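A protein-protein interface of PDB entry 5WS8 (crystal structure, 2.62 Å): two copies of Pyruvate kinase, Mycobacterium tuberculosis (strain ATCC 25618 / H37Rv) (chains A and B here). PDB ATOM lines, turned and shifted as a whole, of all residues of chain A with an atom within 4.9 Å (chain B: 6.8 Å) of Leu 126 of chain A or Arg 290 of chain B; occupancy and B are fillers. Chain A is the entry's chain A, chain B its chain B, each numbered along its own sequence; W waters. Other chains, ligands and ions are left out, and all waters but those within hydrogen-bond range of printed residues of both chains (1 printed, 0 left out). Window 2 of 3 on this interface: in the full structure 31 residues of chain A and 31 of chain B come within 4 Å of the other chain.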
ATOM      1  N   ARG A 124      19.988  15.607  35.930  1.00  0.00           N
ATOM      2  CA  ARG A 124      19.544  15.433  34.555  1.00  0.00           C
ATOM      3  C   ARG A 124      19.421  16.788  33.846  1.00  0.00           C
ATOM      4  O   ARG A 124      19.033  17.798  34.462  1.00  0.00           O
ATOM      5  CB  ARG A 124      18.170  14.772  34.555  1.00  0.00           C
ATOM      6  CG  ARG A 124      18.125  13.376  33.993  1.00  0.00           C
ATOM      7  CD  ARG A 124      17.965  12.324  35.073  1.00  0.00           C
ATOM      8  NE  ARG A 124      18.249  11.003  34.505  1.00  0.00           N
ATOM      9  CZ  ARG A 124      19.184  10.146  34.937  1.00  0.00           C
ATOM     10  NH1 ARG A 124      19.954  10.417  35.996  1.00  0.00           N
ATOM     11  NH2 ARG A 124      19.339   8.997  34.302  1.00  0.00           N
ATOM     12  N   VAL A 125      19.721  16.802  32.554  1.00  0.00           N
ATOM     13  CA  VAL A 125      19.575  18.005  31.780  1.00  0.00           C
ATOM     14  C   VAL A 125      18.767  17.705  30.562  1.00  0.00           C
ATOM     15  O   VAL A 125      19.184  16.943  29.730  1.00  0.00           O
ATOM     16  CB  VAL A 125      20.916  18.559  31.307  1.00  0.00           C
ATOM     17  CG1 VAL A 125      20.685  19.770  30.423  1.00  0.00           C
ATOM     18  CG2 VAL A 125      21.820  18.895  32.479  1.00  0.00           C
ATOM     19  N   LEU A 126      17.603  18.318  30.450  1.00  0.00           N
ATOM     20  CA  LEU A 126      16.766  18.079  29.306  1.00  0.00           C
ATOM     21  C   LEU A 126      16.731  19.297  28.418  1.00  0.00           C
ATOM     22  O   LEU A 126      16.554  20.417  28.873  1.00  0.00           O
ATOM     23  CB  LEU A 126      15.388  17.670  29.756  1.00  0.00           C
ATOM     24  CG  LEU A 126      15.477  16.524  30.755  1.00  0.00           C
ATOM     25  CD1 LEU A 126      14.209  16.454  31.587  1.00  0.00           C
ATOM     26  CD2 LEU A 126      15.731  15.199  30.064  1.00  0.00           C
ATOM     27  N   VAL A 127      16.928  19.072  27.135  1.00  0.00           N
ATOM     28  CA  VAL A 127      17.027  20.161  26.195  1.00  0.00           C
ATOM     29  C   VAL A 127      15.780  20.142  25.329  1.00  0.00           C
ATOM     30  O   VAL A 127      15.304  19.059  24.962  1.00  0.00           O
ATOM     31  CB  VAL A 127      18.286  19.998  25.318  1.00  0.00           C
ATOM     32  CG1 VAL A 127      18.513  21.234  24.482  1.00  0.00           C
ATOM     33  CG2 VAL A 127      19.494  19.756  26.185  1.00  0.00           C
ATOM     34  N   ASP A 128      15.260  21.335  25.006  1.00  0.00           N
ATOM     35  CA  ASP A 128      14.158  21.479  24.054  1.00  0.00           C
ATOM     36  C   ASP A 128      12.974  20.578  24.442  1.00  0.00           C
ATOM     37  O   ASP A 128      12.391  19.903  23.577  1.00  0.00           O
ATOM     38  CB  ASP A 128      14.624  21.140  22.624  1.00  0.00           C
ATOM     39  CG  ASP A 128      13.576  21.517  21.546  1.00  0.00           C
ATOM     40  OD1 ASP A 128      13.088  22.660  21.546  1.00  0.00           O
ATOM     41  OD2 ASP A 128      13.227  20.677  20.695  1.00  0.00           O
ATOM     42  N   GLY A 130      12.791  17.697  26.092  1.00  0.00           N
ATOM     43  CA  GLY A 130      12.983  16.225  26.071  1.00  0.00           C
ATOM     44  C   GLY A 130      13.436  15.619  24.742  1.00  0.00           C
ATOM     45  O   GLY A 130      13.308  14.423  24.527  1.00  0.00           O
ATOM     46  N   VAL A 132      16.603  15.866  23.801  1.00  0.00           N
ATOM     47  CA  VAL A 132      17.967  15.473  24.103  1.00  0.00           C
ATOM     48  C   VAL A 132      18.120  15.500  25.610  1.00  0.00           C
ATOM     49  O   VAL A 132      17.661  16.446  26.270  1.00  0.00           O
ATOM     50  CB  VAL A 132      18.988  16.476  23.521  1.00  0.00           C
ATOM     51  CG1 VAL A 132      20.365  16.256  24.107  1.00  0.00           C
ATOM     52  CG2 VAL A 132      19.037  16.359  22.016  1.00  0.00           C
ATOM     53  N   ALA A 133      18.774  14.469  26.154  1.00  0.00           N
ATOM     54  CA  ALA A 133      18.941  14.312  27.591  1.00  0.00           C
ATOM     55  C   ALA A 133      20.412  14.124  27.937  1.00  0.00           C
ATOM     56  O   ALA A 133      21.168  13.526  27.189  1.00  0.00           O
ATOM     57  CB  ALA A 133      18.139  13.132  28.059  1.00  0.00           C
ATOM     58  N   GLU A 150      20.651  10.711  25.816  1.00  0.00           N
ATOM     59  CA  GLU A 150      19.777  10.556  24.650  1.00  0.00           C
ATOM     60  C   GLU A 150      20.142  11.672  23.699  1.00  0.00           C
ATOM     61  O   GLU A 150      20.080  12.846  24.066  1.00  0.00           O
ATOM     62  CB  GLU A 150      18.312  10.667  25.053  1.00  0.00           C
ATOM     63  CG  GLU A 150      17.823   9.528  25.922  1.00  0.00           C
ATOM     64  CD  GLU A 150      16.515   9.843  26.599  1.00  0.00           C
ATOM     65  OE1 GLU A 150      16.347   9.482  27.781  1.00  0.00           O
ATOM     66  OE2 GLU A 150      15.658  10.478  25.959  1.00  0.00           O
ATOM     67  N   GLY A 159      16.306  25.892  24.988  1.00  0.00           N
ATOM     68  CA  GLY A 159      15.985  25.905  26.397  1.00  0.00           C
ATOM     69  C   GLY A 159      16.318  24.604  27.069  1.00  0.00           C
ATOM     70  O   GLY A 159      16.011  23.519  26.563  1.00  0.00           O
ATOM     71  N   ILE A 160      16.921  24.700  28.238  1.00  0.00           N
ATOM     72  CA  ILE A 160      17.226  23.514  28.990  1.00  0.00           C
ATOM     73  C   ILE A 160      16.522  23.567  30.302  1.00  0.00           C
ATOM     74  O   ILE A 160      16.218  24.625  30.811  1.00  0.00           O
ATOM     75  CB  ILE A 160      18.747  23.342  29.220  1.00  0.00           C
ATOM     76  CG1 ILE A 160      19.229  24.315  30.282  1.00  0.00           C
ATOM     77  CG2 ILE A 160      19.493  23.480  27.895  1.00  0.00           C
ATOM     78  CD1 ILE A 160      20.536  24.983  29.962  1.00  0.00           C
ATOM     79  N   SER A 161      16.274  22.396  30.846  1.00  0.00           N
ATOM     80  CA  SER A 161      15.583  22.267  32.099  1.00  0.00           C
ATOM     81  C   SER A 161      16.375  21.294  32.942  1.00  0.00           C
ATOM     82  O   SER A 161      16.866  20.303  32.436  1.00  0.00           O
ATOM     83  CB  SER A 161      14.177  21.745  31.858  1.00  0.00           C
ATOM     84  OG  SER A 161      13.342  22.182  32.894  1.00  0.00           O
ATOM     85  N   PRO A 163      15.542  19.119  35.938  1.00  0.00           N
ATOM     86  CA  PRO A 163      14.544  18.643  36.905  1.00  0.00           C
ATOM     87  C   PRO A 163      15.097  18.497  38.323  1.00  0.00           C
ATOM     88  O   PRO A 163      16.201  17.992  38.509  1.00  0.00           O
ATOM     89  CB  PRO A 163      14.123  17.276  36.349  1.00  0.00           C
ATOM     90  CG  PRO A 163      14.474  17.321  34.912  1.00  0.00           C
ATOM     91  CD  PRO A 163      15.690  18.197  34.806  1.00  0.00           C
ATOM     92  N   VAL A 250       8.788  18.180  31.710  1.00  0.00           N
ATOM     93  CA  VAL A 250      10.202  17.987  31.929  1.00  0.00           C
ATOM     94  C   VAL A 250      10.599  18.436  33.313  1.00  0.00           C
ATOM     95  O   VAL A 250      11.523  17.880  33.895  1.00  0.00           O
ATOM     96  CB  VAL A 250      11.085  18.665  30.850  1.00  0.00           C
ATOM     97  CG1 VAL A 250      10.869  18.009  29.498  1.00  0.00           C
ATOM     98  CG2 VAL A 250      10.804  20.147  30.727  1.00  0.00           C
ATOM     99  N   LEU A 254       6.758  13.077  33.264  1.00  0.00           N
ATOM    100  CA  LEU A 254       5.686  13.272  32.289  1.00  0.00           C
ATOM    101  C   LEU A 254       4.453  12.431  32.614  1.00  0.00           C
ATOM    102  O   LEU A 254       3.346  12.765  32.209  1.00  0.00           O
ATOM    103  CB  LEU A 254       6.167  13.004  30.861  1.00  0.00           C
ATOM    104  CG  LEU A 254       6.661  11.589  30.542  1.00  0.00           C
ATOM    105  CD1 LEU A 254       5.487  10.714  30.137  1.00  0.00           C
ATOM    106  CD2 LEU A 254       7.702  11.623  29.434  1.00  0.00           C
ATOM    107  N   SER B 284       4.467   8.633  18.720  1.00  0.00           N
ATOM    108  CA  SER B 284       5.704   9.325  18.467  1.00  0.00           C
ATOM    109  C   SER B 284       6.918   8.551  18.958  1.00  0.00           C
ATOM    110  O   SER B 284       8.049   8.905  18.623  1.00  0.00           O
ATOM    111  CB  SER B 284       5.690  10.712  19.106  1.00  0.00           C
ATOM    112  OG  SER B 284       5.801  10.627  20.511  1.00  0.00           O
ATOM    113  N   MET B 285       6.710   7.508  19.756  1.00  0.00           N
ATOM    114  CA  MET B 285       7.854   6.743  20.292  1.00  0.00           C
ATOM    115  C   MET B 285       8.397   5.742  19.293  1.00  0.00           C
ATOM    116  O   MET B 285       9.352   5.021  19.572  1.00  0.00           O
ATOM    117  CB  MET B 285       7.502   6.062  21.611  1.00  0.00           C
ATOM    118  CG  MET B 285       7.425   7.063  22.753  1.00  0.00           C
ATOM    119  SD  MET B 285       7.248   6.306  24.357  1.00  0.00           S
ATOM    120  CE  MET B 285       8.933   5.741  24.618  1.00  0.00           C
ATOM    121  N   GLU B 287       9.782   7.029  16.766  1.00  0.00           N
ATOM    122  CA  GLU B 287      11.028   7.773  16.444  1.00  0.00           C
ATOM    123  C   GLU B 287      11.716   8.376  17.651  1.00  0.00           C
ATOM    124  O   GLU B 287      12.912   8.643  17.602  1.00  0.00           O
ATOM    125  CB  GLU B 287      10.763   8.910  15.463  1.00  0.00           C
ATOM    126  CG  GLU B 287       9.992   8.525  14.216  1.00  0.00           C
ATOM    127  CD  GLU B 287      10.841   7.816  13.189  1.00  0.00           C
ATOM    128  OE1 GLU B 287      10.274   6.977  12.449  1.00  0.00           O
ATOM    129  OE2 GLU B 287      12.065   8.086  13.117  1.00  0.00           O
ATOM    130  N   ASN B 288      10.964   8.628  18.717  1.00  0.00           N
ATOM    131  CA  ASN B 288      11.479   9.401  19.860  1.00  0.00           C
ATOM    132  C   ASN B 288      11.470   8.630  21.170  1.00  0.00           C
ATOM    133  O   ASN B 288      10.564   7.819  21.438  1.00  0.00           O
ATOM    134  CB  ASN B 288      10.644  10.654  20.047  1.00  0.00           C
ATOM    135  CG  ASN B 288      10.575  11.477  18.791  1.00  0.00           C
ATOM    136  OD1 ASN B 288      11.531  12.108  18.402  1.00  0.00           O
ATOM    137  ND2 ASN B 288       9.468  11.416  18.130  1.00  0.00           N
ATOM    138  N   SER B 289      12.453   8.924  22.015  1.00  0.00           N
ATOM    139  CA  SER B 289      12.606   8.213  23.273  1.00  0.00           C
ATOM    140  C   SER B 289      11.551   8.603  24.325  1.00  0.00           C
ATOM    141  O   SER B 289      11.372   7.897  25.323  1.00  0.00           O
ATOM    142  CB  SER B 289      14.002   8.442  23.830  1.00  0.00           C
ATOM    143  OG  SER B 289      14.149   9.759  24.336  1.00  0.00           O
ATOM    144  N   ARG B 290      10.880   9.728  24.123  1.00  0.00           N
ATOM    145  CA  ARG B 290       9.822  10.167  25.034  1.00  0.00           C
ATOM    146  C   ARG B 290       8.614  10.526  24.229  1.00  0.00           C
ATOM    147  O   ARG B 290       8.750  11.045  23.145  1.00  0.00           O
ATOM    148  CB  ARG B 290      10.251  11.405  25.806  1.00  0.00           C
ATOM    149  CG  ARG B 290      11.188  11.156  26.961  1.00  0.00           C
ATOM    150  CD  ARG B 290      11.864  12.466  27.270  1.00  0.00           C
ATOM    151  NE  ARG B 290      12.473  12.550  28.575  1.00  0.00           N
ATOM    152  CZ  ARG B 290      13.637  11.994  28.898  1.00  0.00           C
ATOM    153  NH1 ARG B 290      14.143  12.166  30.122  1.00  0.00           N
ATOM    154  NH2 ARG B 290      14.291  11.250  28.010  1.00  0.00           N
ATOM    155  N   PRO B 291       7.427  10.312  24.773  1.00  0.00           N
ATOM    156  CA  PRO B 291       6.203  10.596  24.038  1.00  0.00           C
ATOM    157  C   PRO B 291       5.782  12.064  24.107  1.00  0.00           C
ATOM    158  O   PRO B 291       6.455  12.879  24.773  1.00  0.00           O
ATOM    159  CB  PRO B 291       5.184   9.733  24.748  1.00  0.00           C
ATOM    160  CG  PRO B 291       5.638   9.746  26.159  1.00  0.00           C
ATOM    161  CD  PRO B 291       7.151   9.862  26.139  1.00  0.00           C
ATOM    162  N   THR B 292       4.685  12.399  23.429  1.00  0.00           N
ATOM    163  CA  THR B 292       4.136  13.748  23.516  1.00  0.00           C
ATOM    164  C   THR B 292       3.193  13.897  24.689  1.00  0.00           C
ATOM    165  O   THR B 292       2.679  12.924  25.249  1.00  0.00           O
ATOM    166  CB  THR B 292       3.378  14.169  22.246  1.00  0.00           C
ATOM    167  OG1 THR B 292       2.182  13.385  22.088  1.00  0.00           O
ATOM    168  CG2 THR B 292       4.247  14.030  21.015  1.00  0.00           C
ATOM    169  N   ARG B 293       2.906  15.134  25.029  1.00  0.00           N
ATOM    170  CA  ARG B 293       2.001  15.381  26.104  1.00  0.00           C
ATOM    171  C   ARG B 293       0.609  14.821  25.782  1.00  0.00           C
ATOM    172  O   ARG B 293      -0.120  14.399  26.676  1.00  0.00           O
ATOM    173  CB  ARG B 293       1.950  16.868  26.415  1.00  0.00           C
ATOM    174  CG  ARG B 293       3.306  17.480  26.769  1.00  0.00           C
ATOM    175  CD  ARG B 293       3.880  16.943  28.075  1.00  0.00           C
ATOM    176  NE  ARG B 293       5.192  17.512  28.247  1.00  0.00           N
ATOM    177  CZ  ARG B 293       6.294  17.018  27.713  1.00  0.00           C
ATOM    178  NH1 ARG B 293       6.273  15.883  27.041  1.00  0.00           N
ATOM    179  NH2 ARG B 293       7.421  17.661  27.858  1.00  0.00           N
ATOM    180  N   GLU B 295       0.091  12.147  23.985  1.00  0.00           N
ATOM    181  CA  GLU B 295       0.176  10.719  24.083  1.00  0.00           C
ATOM    182  C   GLU B 295       0.088  10.268  25.541  1.00  0.00           C
ATOM    183  O   GLU B 295      -0.738   9.428  25.877  1.00  0.00           O
ATOM    184  CB  GLU B 295       1.421  10.232  23.376  1.00  0.00           C
ATOM    185  CG  GLU B 295       1.205  10.255  21.881  1.00  0.00           C
ATOM    186  CD  GLU B 295       2.469  10.242  21.059  1.00  0.00           C
ATOM    187  OE1 GLU B 295       3.584  10.326  21.643  1.00  0.00           O
ATOM    188  OE2 GLU B 295       2.319  10.171  19.802  1.00  0.00           O
ATOM    189  N   TYR B 321      12.214   2.193  19.799  1.00  0.00           N
ATOM    190  CA  TYR B 321      12.194   2.123  21.253  1.00  0.00           C
ATOM    191  C   TYR B 321      11.107   1.207  21.788  1.00  0.00           C
ATOM    192  O   TYR B 321      10.304   1.621  22.617  1.00  0.00           O
ATOM    193  CB  TYR B 321      12.012   3.514  21.844  1.00  0.00           C
ATOM    194  CG  TYR B 321      13.063   4.512  21.411  1.00  0.00           C
ATOM    195  CD1 TYR B 321      14.218   4.709  22.164  1.00  0.00           C
ATOM    196  CD2 TYR B 321      12.885   5.285  20.271  1.00  0.00           C
ATOM    197  CE1 TYR B 321      15.167   5.628  21.785  1.00  0.00           C
ATOM    198  CE2 TYR B 321      13.838   6.210  19.888  1.00  0.00           C
ATOM    199  CZ  TYR B 321      14.966   6.376  20.649  1.00  0.00           C
ATOM    200  OH  TYR B 321      15.902   7.290  20.294  1.00  0.00           O
ATOM    201  N   ALA B 324      11.309   0.869  25.718  1.00  0.00           N
ATOM    202  CA  ALA B 324      10.987   2.095  26.402  1.00  0.00           C
ATOM    203  C   ALA B 324       9.510   2.398  26.283  1.00  0.00           C
ATOM    204  O   ALA B 324       8.929   2.969  27.191  1.00  0.00           O
ATOM    205  CB  ALA B 324      11.792   3.249  25.840  1.00  0.00           C
ATOM    206  N   THR B 328       7.341   3.039  29.413  1.00  0.00           N
ATOM    207  CA  THR B 328       6.676   4.320  29.510  1.00  0.00           C
ATOM    208  C   THR B 328       5.174   4.145  29.645  1.00  0.00           C
ATOM    209  O   THR B 328       4.547   4.831  30.429  1.00  0.00           O
ATOM    210  CB  THR B 328       6.962   5.170  28.287  1.00  0.00           C
ATOM    211  OG1 THR B 328       8.360   5.462  28.251  1.00  0.00           O
ATOM    212  CG2 THR B 328       6.169   6.453  28.332  1.00  0.00           C
HETATM  213  O   HOH W   1      16.497  11.981  31.937  1.00  0.00           O
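The side-chain hydroxyl of Ser 289 of chain B sits close to the side-chain carboxylate of Glu 150 of chain A (2.3 Å).
OE2 of Glu 150 of chain A is in salt-bridge range of NH2 of Arg 290 of chain B, at 2.6 Å.
The backbone NH (N) of Ala 133 of chain A sits at hydrogen-bond distance from the backbone carbonyl oxygen (O) of Glu 150 of chain A (2.9 Å).
N of Ser 161 of chain A is in hydrogen-bond range of O of Leu 126 of chain A.
Leu 126 of chain A touches Arg 290 of chain B (CD2 to NH1, 3.4 Å).
Gly 130 of chain A touches Arg 290 of chain B (O to CD, 3.7 Å).
Val 250 of chain A touches Arg 293 of chain B.
CD of Pro 291 of chain B touches CD2 of Leu 254 of chain A, 3.8 Å away.
Leu 126 of chain A touches just one residue of chain B: Arg 290.
Of the printed residues of chain B, Gly 130 of chain A touches Arg 290.
Val 132 of chain A touches none of the printed residues of chain B.
Arg 290 of chain B touches just these residues of chain A: Leu 126, Gly 130 and Glu 150.
Printed residues of chain A within 4 Å of Pro 291 of chain B: Leu 254 (3.8 Å).
Printed residues of chain A within 4 Å of Arg 293 of chain B: Val 250.
Tyr 321 of chain B touches none of the printed residues of chain A.
The nearest printed residue of chain A that does not touch Arg 290 of chain B is Ala 133 of chain A (4.3 Å).
The nearest printed residue of chain A that does not touch Pro 291 of chain B is Gly 130 of chain A (7.0 Å).
Of the 13 printed residues of chain B, 4 touch a printed residue of chain A.
Among the printed residues, Asp or Glu carboxylates within 4 Å of a Lys or Arg side-chain nitrogen of the other chain: Glu 150 of chain A with Arg 290 of chain B (2.6 Å).
No position is printed for both chains.
Of the 6 pairs that touch across the chains among the printed residues, none has its exchanged pair printed and touching as well.
Water W1 bridges NH1 of Arg 290 of chain B and NE of Arg 124 of chain A.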
